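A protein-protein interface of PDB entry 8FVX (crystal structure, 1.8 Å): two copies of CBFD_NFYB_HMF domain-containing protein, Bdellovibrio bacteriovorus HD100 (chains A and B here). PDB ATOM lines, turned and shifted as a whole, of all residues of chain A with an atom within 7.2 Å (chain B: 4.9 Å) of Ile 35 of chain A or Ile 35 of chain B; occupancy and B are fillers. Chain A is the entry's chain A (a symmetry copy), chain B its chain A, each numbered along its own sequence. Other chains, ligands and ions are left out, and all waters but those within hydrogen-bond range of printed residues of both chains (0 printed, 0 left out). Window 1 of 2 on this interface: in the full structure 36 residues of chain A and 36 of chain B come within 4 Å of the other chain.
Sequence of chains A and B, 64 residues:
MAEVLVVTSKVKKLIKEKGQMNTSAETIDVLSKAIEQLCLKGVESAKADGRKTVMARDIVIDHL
Leu 5 of chain A touches Val 6 of chain B (O to CA, 3.4 Å). Val 6 of chain A touches Leu 5 of chain B (CA to O, 3.4 Å). Ile 35 of chain B touches Val 6 of chain A. O of Val 6 of chain B touches CG2 of Val 7 of chain A (3.5 Å). CG2 of Ile 35 of chain B touches CG2 of Val 11 of chain A, 3.9 Å away. Leu 31 of chain A touches Cys 39 of chain B. Ile 35 of chain A touches Val 11 of chain B (CG2 to CG2, 3.9 Å). Ile 35 of chain A touches Ile 35 of chain B. Cys 39 of chain A touches Val 11 of chain B (SG to CG1, 3.7 Å). Ala 34 of chain B touches Leu 64 of chain A (O to CD2, 3.7 Å).
Val 6 of chain A touches Ile 35 of chain B, and with the chains exchanged Ile 35 of chain A touches Val 6 of chain B. Val 11 of chain A touches Cys 39 of chain B, and with the chains exchanged Cys 39 of chain A touches Val 11 of chain B. Leu 31 of chain A touches Ile 35 of chain B, and with the chains exchanged Ile 35 of chain A touches Leu 31 of chain B. Leu 31 of chain A touches Leu 38 of chain B, and with the chains exchanged Leu 38 of chain A touches Leu 31 of chain B. Positions printed for both chains: 5, 6, 11, 31, 32, 33, 34, 35, 36, 37, 38 and 39.
Hydrophobic or aromatic side chains of chain A within 4 Å of the printed part of chain B: Val 6, Val 7, Val 11, Leu 14, Ile 15, Leu 31, Ile 35, Leu 38 and Leu 64. Printed residues of chain B that touch a printed residue of chain A: Leu 5, Val 6, Val 11, Leu 31, Ala 34, Ile 35, Leu 38 and Cys 39. Hydrophobic or aromatic side chains of chain B within 4 Å of the printed part of chain A: Val 6, Val 11, Leu 31, Ile 35 and Leu 38. Among the printed residues, 21 pairs touch across the chains. Among the printed residues, no Asp or Glu carboxylate lies within 4 Å of a Lys or Arg side-chain nitrogen of the other chain.
Of chain B, only Val 6, Val 11, Leu 31 and Ile 35 come within 4 Å of Ile 35 of chain A. Of chain A, only Val 6, Val 11, Leu 31 and Ile 35 come within 4 Å of Ile 35 of chain B. Of the printed residues of chain B, Leu 5 of chain A touches Val 6. Of the printed residues of chain B, Val 7 of chain A touches Leu 5 (3.0 Å) and Val 6 (3.5 Å). Of the printed residues of chain A, Leu 38 of chain B touches Leu 31 (3.9 Å) and Leu 64 (3.9 Å). Of the printed residues of chain B, Cys 39 of chain A touches Val 11 (3.7 Å) and Leu 31 (3.9 Å). Printed residues of chain A within 4 Å of Val 6 of chain B: Leu 5 (3.4 Å), Val 7 (3.5 Å) and Ile 35 (3.9 Å).
The backbone NH (N) of Leu 5 of chain B lies within hydrogen-bond range of the side-chain hydroxyl (OG) of Ser 32 of chain B (2.9 Å). The backbone carbonyl oxygen (O) of Ile 35 of chain B is in hydrogen-bond range of the side-chain sulfur (SG) of Cys 39 of chain B (3.2 Å). N of Leu 5 of chain A sits at hydrogen-bond distance from OG of Ser 32 of chain A (2.9 Å). The backbone carbonyl oxygen (O) of Ile 35 of chain A sits at hydrogen-bond distance from the side-chain sulfur (SG) of Cys 39 of chain A.
The backbone NH of Val 7 of chain A lies within hydrogen-bond range of the backbone carbonyl oxygen of Leu 5 of chain B.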
ATOM      1  N   LEU A   5       2.255  19.188 -16.190  1.00  0.00           N
ATOM      2  CA  LEU A   5       3.048  19.597 -17.352  1.00  0.00           C
ATOM      3  C   LEU A   5       4.506  19.151 -17.297  1.00  0.00           C
ATOM      4  O   LEU A   5       5.259  19.449 -18.228  1.00  0.00           O
ATOM      5  CB  LEU A   5       2.994  21.119 -17.520  1.00  0.00           C
ATOM      6  CG  LEU A   5       1.583  21.697 -17.664  1.00  0.00           C
ATOM      7  CD1 LEU A   5       1.635  23.210 -17.702  1.00  0.00           C
ATOM      8  CD2 LEU A   5       0.880  21.137 -18.894  1.00  0.00           C
ATOM      9  N   VAL A   6       4.938  18.469 -16.238  1.00  0.00           N
ATOM     10  CA  VAL A   6       6.268  17.869 -16.213  1.00  0.00           C
ATOM     11  C   VAL A   6       6.113  16.359 -16.298  1.00  0.00           C
ATOM     12  O   VAL A   6       5.073  15.797 -15.936  1.00  0.00           O
ATOM     13  CB  VAL A   6       7.104  18.255 -14.972  1.00  0.00           C
ATOM     14  CG1 VAL A   6       7.382  19.775 -14.959  1.00  0.00           C
ATOM     15  CG2 VAL A   6       6.416  17.783 -13.708  1.00  0.00           C
ATOM     16  N   VAL A   7       7.153  15.704 -16.812  1.00  0.00           N
ATOM     17  CA  VAL A   7       7.167  14.245 -16.922  1.00  0.00           C
ATOM     18  C   VAL A   7       7.563  13.698 -15.554  1.00  0.00           C
ATOM     19  O   VAL A   7       8.748  13.584 -15.233  1.00  0.00           O
ATOM     20  CB  VAL A   7       8.104  13.766 -18.033  1.00  0.00           C
ATOM     21  CG1 VAL A   7       7.959  12.272 -18.230  1.00  0.00           C
ATOM     22  CG2 VAL A   7       7.783  14.500 -19.325  1.00  0.00           C
ATOM     23  N   VAL A  11      11.382  13.275 -13.853  1.00  0.00           N
ATOM     24  CA  VAL A  11      11.810  14.172 -12.783  1.00  0.00           C
ATOM     25  C   VAL A  11      12.249  13.372 -11.561  1.00  0.00           C
ATOM     26  O   VAL A  11      13.336  13.600 -11.011  1.00  0.00           O
ATOM     27  CB  VAL A  11      10.683  15.159 -12.429  1.00  0.00           C
ATOM     28  CG1 VAL A  11      10.941  15.786 -11.071  1.00  0.00           C
ATOM     29  CG2 VAL A  11      10.530  16.220 -13.524  1.00  0.00           C
ATOM     30  N   LEU A  14      15.598  11.759 -12.293  1.00  0.00           N
ATOM     31  CA  LEU A  14      16.722  12.686 -12.223  1.00  0.00           C
ATOM     32  C   LEU A  14      17.109  12.955 -10.778  1.00  0.00           C
ATOM     33  O   LEU A  14      18.294  12.924 -10.417  1.00  0.00           O
ATOM     34  CB  LEU A  14      16.359  14.004 -12.919  1.00  0.00           C
ATOM     35  CG  LEU A  14      17.381  15.140 -12.739  1.00  0.00           C
ATOM     36  CD1 LEU A  14      18.722  14.807 -13.415  1.00  0.00           C
ATOM     37  CD2 LEU A  14      16.841  16.458 -13.268  1.00  0.00           C
ATOM     38  N   ILE A  15      16.112  13.233  -9.941  1.00  0.00           N
ATOM     39  CA  ILE A  15      16.376  13.621  -8.563  1.00  0.00           C
ATOM     40  C   ILE A  15      16.963  12.455  -7.784  1.00  0.00           C
ATOM     41  O   ILE A  15      17.854  12.639  -6.947  1.00  0.00           O
ATOM     42  CB  ILE A  15      15.085  14.157  -7.927  1.00  0.00           C
ATOM     43  CG1 ILE A  15      14.789  15.542  -8.492  1.00  0.00           C
ATOM     44  CG2 ILE A  15      15.199  14.173  -6.404  1.00  0.00           C
ATOM     45  CD1 ILE A  15      13.391  16.048  -8.169  1.00  0.00           C
ATOM     46  N   ASP A  29       3.910  19.211  -8.206  1.00  0.00           N
ATOM     47  CA  ASP A  29       2.925  20.269  -8.412  1.00  0.00           C
ATOM     48  C   ASP A  29       3.600  21.611  -8.648  1.00  0.00           C
ATOM     49  O   ASP A  29       3.210  22.361  -9.546  1.00  0.00           O
ATOM     50  CB  ASP A  29       1.986  20.367  -7.213  1.00  0.00           C
ATOM     51  CG  ASP A  29       0.967  19.239  -7.168  1.00  0.00           C
ATOM     52  OD1 ASP A  29       0.734  18.595  -8.212  1.00  0.00           O
ATOM     53  OD2 ASP A  29       0.411  18.989  -6.083  1.00  0.00           O
ATOM     54  N   VAL A  30       4.605  21.941  -7.832  1.00  0.00           N
ATOM     55  CA  VAL A  30       5.293  23.223  -7.991  1.00  0.00           C
ATOM     56  C   VAL A  30       5.934  23.306  -9.369  1.00  0.00           C
ATOM     57  O   VAL A  30       5.818  24.316 -10.071  1.00  0.00           O
ATOM     58  CB  VAL A  30       6.338  23.413  -6.879  1.00  0.00           C
ATOM     59  CG1 VAL A  30       7.214  24.647  -7.159  1.00  0.00           C
ATOM     60  CG2 VAL A  30       5.640  23.550  -5.535  1.00  0.00           C
ATOM     61  N   LEU A  31       6.645  22.252  -9.762  1.00  0.00           N
ATOM     62  CA  LEU A  31       7.290  22.250 -11.071  1.00  0.00           C
ATOM     63  C   LEU A  31       6.270  22.432 -12.186  1.00  0.00           C
ATOM     64  O   LEU A  31       6.501  23.193 -13.129  1.00  0.00           O
ATOM     65  CB  LEU A  31       8.077  20.954 -11.270  1.00  0.00           C
ATOM     66  CG  LEU A  31       9.298  20.749 -10.372  1.00  0.00           C
ATOM     67  CD1 LEU A  31       9.767  19.299 -10.454  1.00  0.00           C
ATOM     68  CD2 LEU A  31      10.416  21.719 -10.798  1.00  0.00           C
ATOM     69  N   SER A  32       5.127  21.753 -12.086  1.00  0.00           N
ATOM     70  CA  SER A  32       4.089  21.908 -13.095  1.00  0.00           C
ATOM     71  C   SER A  32       3.569  23.345 -13.149  1.00  0.00           C
ATOM     72  O   SER A  32       3.416  23.916 -14.237  1.00  0.00           O
ATOM     73  CB  SER A  32       2.951  20.930 -12.813  1.00  0.00           C
ATOM     74  OG  SER A  32       2.046  20.914 -13.893  1.00  0.00           O
ATOM     75  N   LYS A  33       3.274  23.942 -11.982  1.00  0.00           N
ATOM     76  CA  LYS A  33       2.777  25.319 -11.955  1.00  0.00           C
ATOM     77  C   LYS A  33       3.818  26.294 -12.488  1.00  0.00           C
ATOM     78  O   LYS A  33       3.479  27.266 -13.178  1.00  0.00           O
ATOM     79  CB  LYS A  33       2.359  25.723 -10.534  1.00  0.00           C
ATOM     80  CG  LYS A  33       1.077  25.073 -10.018  1.00  0.00           C
ATOM     81  CD  LYS A  33      -0.040  25.210 -11.031  1.00  0.00           C
ATOM     82  CE  LYS A  33      -0.823  26.507 -10.835  1.00  0.00           C
ATOM     83  NZ  LYS A  33      -2.293  26.262 -10.720  1.00  0.00           N
ATOM     84  N   ALA A  34       5.095  26.036 -12.200  1.00  0.00           N
ATOM     85  CA  ALA A  34       6.171  26.857 -12.751  1.00  0.00           C
ATOM     86  C   ALA A  34       6.191  26.801 -14.276  1.00  0.00           C
ATOM     87  O   ALA A  34       6.357  27.834 -14.942  1.00  0.00           O
ATOM     88  CB  ALA A  34       7.518  26.402 -12.185  1.00  0.00           C
ATOM     89  N   ILE A  35       6.011  25.610 -14.849  1.00  0.00           N
ATOM     90  CA  ILE A  35       5.959  25.478 -16.307  1.00  0.00           C
ATOM     91  C   ILE A  35       4.762  26.234 -16.873  1.00  0.00           C
ATOM     92  O   ILE A  35       4.858  26.898 -17.913  1.00  0.00           O
ATOM     93  CB  ILE A  35       5.930  23.987 -16.700  1.00  0.00           C
ATOM     94  CG1 ILE A  35       7.297  23.363 -16.447  1.00  0.00           C
ATOM     95  CG2 ILE A  35       5.545  23.809 -18.193  1.00  0.00           C
ATOM     96  CD1 ILE A  35       8.425  24.257 -16.915  1.00  0.00           C
ATOM     97  N   GLU A  36       3.609  26.131 -16.214  1.00  0.00           N
ATOM     98  CA  GLU A  36       2.425  26.848 -16.682  1.00  0.00           C
ATOM     99  C   GLU A  36       2.683  28.348 -16.717  1.00  0.00           C
ATOM    100  O   GLU A  36       2.391  29.025 -17.711  1.00  0.00           O
ATOM    101  CB  GLU A  36       1.238  26.526 -15.776  1.00  0.00           C
ATOM    102  CG  GLU A  36      -0.032  27.294 -16.108  1.00  0.00           C
ATOM    103  CD  GLU A  36      -1.175  26.912 -15.188  1.00  0.00           C
ATOM    104  OE1 GLU A  36      -0.954  26.869 -13.965  1.00  0.00           O
ATOM    105  OE2 GLU A  36      -2.285  26.653 -15.681  1.00  0.00           O
ATOM    106  N   GLN A  37       3.264  28.881 -15.646  1.00  0.00           N
ATOM    107  CA  GLN A  37       3.533  30.313 -15.604  1.00  0.00           C
ATOM    108  C   GLN A  37       4.551  30.712 -16.657  1.00  0.00           C
ATOM    109  O   GLN A  37       4.368  31.721 -17.353  1.00  0.00           O
ATOM    110  CB  GLN A  37       3.994  30.706 -14.204  1.00  0.00           C
ATOM    111  CG  GLN A  37       2.834  30.630 -13.211  1.00  0.00           C
ATOM    112  CD  GLN A  37       1.683  31.543 -13.635  1.00  0.00           C
ATOM    113  OE1 GLN A  37       1.880  32.745 -13.815  1.00  0.00           O
ATOM    114  NE2 GLN A  37       0.495  30.971 -13.840  1.00  0.00           N
ATOM    115  N   LEU A  38       5.625  29.928 -16.809  1.00  0.00           N
ATOM    116  CA  LEU A  38       6.609  30.273 -17.831  1.00  0.00           C
ATOM    117  C   LEU A  38       5.971  30.287 -19.214  1.00  0.00           C
ATOM    118  O   LEU A  38       6.293  31.148 -20.040  1.00  0.00           O
ATOM    119  CB  LEU A  38       7.788  29.304 -17.798  1.00  0.00           C
ATOM    120  CG  LEU A  38       8.742  29.465 -16.621  1.00  0.00           C
ATOM    121  CD1 LEU A  38       9.740  28.340 -16.654  1.00  0.00           C
ATOM    122  CD2 LEU A  38       9.443  30.820 -16.711  1.00  0.00           C
ATOM    123  N   CYS A  39       5.047  29.352 -19.476  1.00  0.00           N
ATOM    124  CA  CYS A  39       4.375  29.320 -20.777  1.00  0.00           C
ATOM    125  C   CYS A  39       3.469  30.534 -20.963  1.00  0.00           C
ATOM    126  O   CYS A  39       3.485  31.180 -22.022  1.00  0.00           O
ATOM    127  CB  CYS A  39       3.564  28.028 -20.923  1.00  0.00           C
ATOM    128  SG  CYS A  39       4.533  26.527 -21.109  1.00  0.00           S
ATOM    129  N   LEU A  40       2.654  30.856 -19.950  1.00  0.00           N
ATOM    130  CA  LEU A  40       1.758  32.006 -20.085  1.00  0.00           C
ATOM    131  C   LEU A  40       2.543  33.301 -20.253  1.00  0.00           C
ATOM    132  O   LEU A  40       2.172  34.163 -21.050  1.00  0.00           O
ATOM    133  CB  LEU A  40       0.825  32.094 -18.874  1.00  0.00           C
ATOM    134  CG  LEU A  40      -0.107  30.891 -18.751  1.00  0.00           C
ATOM    135  CD1 LEU A  40      -0.912  30.985 -17.460  1.00  0.00           C
ATOM    136  CD2 LEU A  40      -1.019  30.742 -19.971  1.00  0.00           C
ATOM    137  N   LYS A  41       3.636  33.453 -19.511  1.00  0.00           N
ATOM    138  CA  LYS A  41       4.498  34.610 -19.686  1.00  0.00           C
ATOM    139  C   LYS A  41       5.136  34.618 -21.070  1.00  0.00           C
ATOM    140  O   LYS A  41       5.344  35.690 -21.658  1.00  0.00           O
ATOM    141  CB  LYS A  41       5.566  34.602 -18.581  1.00  0.00           C
ATOM    142  CG  LYS A  41       5.052  35.063 -17.219  1.00  0.00           C
ATOM    143  CD  LYS A  41       6.196  35.610 -16.373  1.00  0.00           C
ATOM    144  CE  LYS A  41       5.706  36.620 -15.343  1.00  0.00           C
ATOM    145  NZ  LYS A  41       4.780  36.007 -14.368  1.00  0.00           N
ATOM    146  N   ILE A  59      10.825  32.825 -23.147  1.00  0.00           N
ATOM    147  CA  ILE A  59      10.811  32.104 -21.867  1.00  0.00           C
ATOM    148  C   ILE A  59      11.960  32.687 -21.050  1.00  0.00           C
ATOM    149  O   ILE A  59      13.119  32.288 -21.182  1.00  0.00           O
ATOM    150  CB  ILE A  59      10.955  30.593 -22.058  1.00  0.00           C
ATOM    151  CG1 ILE A  59       9.919  30.059 -23.061  1.00  0.00           C
ATOM    152  CG2 ILE A  59      10.889  29.862 -20.695  1.00  0.00           C
ATOM    153  CD1 ILE A  59       8.505  30.027 -22.546  1.00  0.00           C
ATOM    154  N   ILE A  61      14.092  32.922 -18.134  1.00  0.00           N
ATOM    155  CA  ILE A  61      14.433  32.079 -16.993  1.00  0.00           C
ATOM    156  C   ILE A  61      15.783  32.485 -16.413  1.00  0.00           C
ATOM    157  O   ILE A  61      16.384  31.724 -15.647  1.00  0.00           O
ATOM    158  CB  ILE A  61      14.433  30.582 -17.369  1.00  0.00           C
ATOM    159  CG1 ILE A  61      14.979  30.328 -18.784  1.00  0.00           C
ATOM    160  CG2 ILE A  61      13.013  30.024 -17.282  1.00  0.00           C
ATOM    161  CD1 ILE A  61      16.450  30.595 -18.969  1.00  0.00           C
ATOM    162  N   LEU A  64      17.088  32.107 -12.805  1.00  0.00           N
ATOM    163  CA  LEU A  64      17.514  30.813 -12.286  1.00  0.00           C
ATOM    164  C   LEU A  64      19.037  30.776 -12.169  1.00  0.00           C
ATOM    165  O   LEU A  64      19.648  29.705 -12.140  1.00  0.00           O
ATOM    166  CB  LEU A  64      17.015  29.686 -13.197  1.00  0.00           C
ATOM    167  CG  LEU A  64      15.720  28.980 -12.798  1.00  0.00           C
ATOM    168  CD1 LEU A  64      14.508  29.824 -13.161  1.00  0.00           C
ATOM    169  CD2 LEU A  64      15.648  27.616 -13.488  1.00  0.00           C
ATOM    170  N   LEU B   5      11.989  16.832 -20.067  1.00  0.00           N
ATOM    171  CA  LEU B   5      11.338  16.765 -18.756  1.00  0.00           C
ATOM    172  C   LEU B   5       9.992  17.480 -18.693  1.00  0.00           C
ATOM    173  O   LEU B   5       9.364  17.484 -17.631  1.00  0.00           O
ATOM    174  CB  LEU B   5      12.262  17.338 -17.677  1.00  0.00           C
ATOM    175  CG  LEU B   5      13.630  16.656 -17.577  1.00  0.00           C
ATOM    176  CD1 LEU B   5      14.504  17.373 -16.570  1.00  0.00           C
ATOM    177  CD2 LEU B   5      13.487  15.179 -17.233  1.00  0.00           C
ATOM    178  N   VAL B   6       9.534  18.101 -19.780  1.00  0.00           N
ATOM    179  CA  VAL B   6       8.182  18.647 -19.828  1.00  0.00           C
ATOM    180  C   VAL B   6       7.354  17.791 -20.773  1.00  0.00           C
ATOM    181  O   VAL B   6       7.884  17.124 -21.669  1.00  0.00           O
ATOM    182  CB  VAL B   6       8.122  20.130 -20.256  1.00  0.00           C
ATOM    183  CG1 VAL B   6       8.845  21.021 -19.220  1.00  0.00           C
ATOM    184  CG2 VAL B   6       8.684  20.298 -21.652  1.00  0.00           C
ATOM    185  N   VAL B  11       2.188  21.121 -23.110  1.00  0.00           N
ATOM    186  CA  VAL B  11       2.699  22.486 -23.196  1.00  0.00           C
ATOM    187  C   VAL B  11       2.208  23.160 -24.473  1.00  0.00           C
ATOM    188  O   VAL B  11       1.681  24.281 -24.436  1.00  0.00           O
ATOM    189  CB  VAL B  11       4.236  22.487 -23.120  1.00  0.00           C
ATOM    190  CG1 VAL B  11       4.787  23.806 -23.631  1.00  0.00           C
ATOM    191  CG2 VAL B  11       4.708  22.192 -21.692  1.00  0.00           C
ATOM    192  N   LEU B  31      12.286  25.053 -21.585  1.00  0.00           N
ATOM    193  CA  LEU B  31      11.456  24.609 -20.469  1.00  0.00           C
ATOM    194  C   LEU B  31      12.032  23.360 -19.819  1.00  0.00           C
ATOM    195  O   LEU B  31      12.074  23.255 -18.591  1.00  0.00           O
ATOM    196  CB  LEU B  31      10.025  24.355 -20.946  1.00  0.00           C
ATOM    197  CG  LEU B  31       9.227  25.577 -21.401  1.00  0.00           C
ATOM    198  CD1 LEU B  31       7.970  25.131 -22.144  1.00  0.00           C
ATOM    199  CD2 LEU B  31       8.870  26.441 -20.177  1.00  0.00           C
ATOM    200  N   SER B  32      12.498  22.409 -20.629  1.00  0.00           N
ATOM    201  CA  SER B  32      13.100  21.203 -20.077  1.00  0.00           C
ATOM    202  C   SER B  32      14.351  21.525 -19.257  1.00  0.00           C
ATOM    203  O   SER B  32      14.525  21.004 -18.148  1.00  0.00           O
ATOM    204  CB  SER B  32      13.429  20.231 -21.207  1.00  0.00           C
ATOM    205  OG  SER B  32      13.807  18.981 -20.678  1.00  0.00           O
ATOM    206  N   LYS B  33      15.245  22.371 -19.797  1.00  0.00           N
ATOM    207  CA  LYS B  33      16.463  22.730 -19.068  1.00  0.00           C
ATOM    208  C   LYS B  33      16.139  23.481 -17.784  1.00  0.00           C
ATOM    209  O   LYS B  33      16.802  23.289 -16.755  1.00  0.00           O
ATOM    210  CB  LYS B  33      17.398  23.572 -19.947  1.00  0.00           C
ATOM    211  CG  LYS B  33      18.096  22.815 -21.075  1.00  0.00           C
ATOM    212  CD  LYS B  33      18.745  21.551 -20.553  1.00  0.00           C
ATOM    213  CE  LYS B  33      20.173  21.806 -20.074  1.00  0.00           C
ATOM    214  NZ  LYS B  33      21.152  20.868 -20.703  1.00  0.00           N
ATOM    215  N   ALA B  34      15.105  24.323 -17.819  1.00  0.00           N
ATOM    216  CA  ALA B  34      14.656  25.012 -16.610  1.00  0.00           C
ATOM    217  C   ALA B  34      14.202  24.024 -15.540  1.00  0.00           C
ATOM    218  O   ALA B  34      14.532  24.184 -14.355  1.00  0.00           O
ATOM    219  CB  ALA B  34      13.522  25.983 -16.952  1.00  0.00           C
ATOM    220  N   ILE B  35      13.457  22.990 -15.935  1.00  0.00           N
ATOM    221  CA  ILE B  35      13.028  21.965 -14.980  1.00  0.00           C
ATOM    222  C   ILE B  35      14.234  21.227 -14.406  1.00  0.00           C
ATOM    223  O   ILE B  35      14.290  20.932 -13.205  1.00  0.00           O
ATOM    224  CB  ILE B  35      12.037  20.997 -15.657  1.00  0.00           C
ATOM    225  CG1 ILE B  35      10.703  21.700 -15.875  1.00  0.00           C
ATOM    226  CG2 ILE B  35      11.820  19.724 -14.795  1.00  0.00           C
ATOM    227  CD1 ILE B  35      10.282  22.508 -14.667  1.00  0.00           C
ATOM    228  N   GLU B  36      15.207  20.896 -15.254  1.00  0.00           N
ATOM    229  CA  GLU B  36      16.404  20.211 -14.772  1.00  0.00           C
ATOM    230  C   GLU B  36      17.117  21.050 -13.719  1.00  0.00           C
ATOM    231  O   GLU B  36      17.484  20.553 -12.647  1.00  0.00           O
ATOM    232  CB  GLU B  36      17.335  19.915 -15.947  1.00  0.00           C
ATOM    233  CG  GLU B  36      18.662  19.288 -15.553  1.00  0.00           C
ATOM    234  CD  GLU B  36      19.527  19.000 -16.765  1.00  0.00           C
ATOM    235  OE1 GLU B  36      19.661  19.896 -17.616  1.00  0.00           O
ATOM    236  OE2 GLU B  36      20.067  17.886 -16.869  1.00  0.00           O
ATOM    237  N   GLN B  37      17.293  22.337 -13.998  1.00  0.00           N
ATOM    238  CA  GLN B  37      17.976  23.200 -13.042  1.00  0.00           C
ATOM    239  C   GLN B  37      17.180  23.334 -11.757  1.00  0.00           C
ATOM    240  O   GLN B  37      17.748  23.252 -10.658  1.00  0.00           O
ATOM    241  CB  GLN B  37      18.243  24.560 -13.679  1.00  0.00           C
ATOM    242  CG  GLN B  37      19.327  24.451 -14.753  1.00  0.00           C
ATOM    243  CD  GLN B  37      20.630  23.906 -14.168  1.00  0.00           C
ATOM    244  OE1 GLN B  37      21.168  24.475 -13.219  1.00  0.00           O
ATOM    245  NE2 GLN B  37      21.114  22.782 -14.701  1.00  0.00           N
ATOM    246  N   LEU B  38      15.860  23.525 -11.863  1.00  0.00           N
ATOM    247  CA  LEU B  38      15.064  23.634 -10.644  1.00  0.00           C
ATOM    248  C   LEU B  38      15.182  22.368  -9.806  1.00  0.00           C
ATOM    249  O   LEU B  38      15.248  22.440  -8.573  1.00  0.00           O
ATOM    250  CB  LEU B  38      13.602  23.921 -10.974  1.00  0.00           C
ATOM    251  CG  LEU B  38      13.300  25.330 -11.467  1.00  0.00           C
ATOM    252  CD1 LEU B  38      11.859  25.391 -11.897  1.00  0.00           C
ATOM    253  CD2 LEU B  38      13.578  26.335 -10.351  1.00  0.00           C
ATOM    254  N   CYS B  39      15.232  21.199 -10.459  1.00  0.00           N
ATOM    255  CA  CYS B  39      15.369  19.943  -9.719  1.00  0.00           C
ATOM    256  C   CYS B  39      16.737  19.841  -9.049  1.00  0.00           C
ATOM    257  O   CYS B  39      16.838  19.476  -7.867  1.00  0.00           O
ATOM    258  CB  CYS B  39      15.147  18.750 -10.654  1.00  0.00           C
ATOM    259  SG  CYS B  39      13.459  18.518 -11.221  1.00  0.00           S
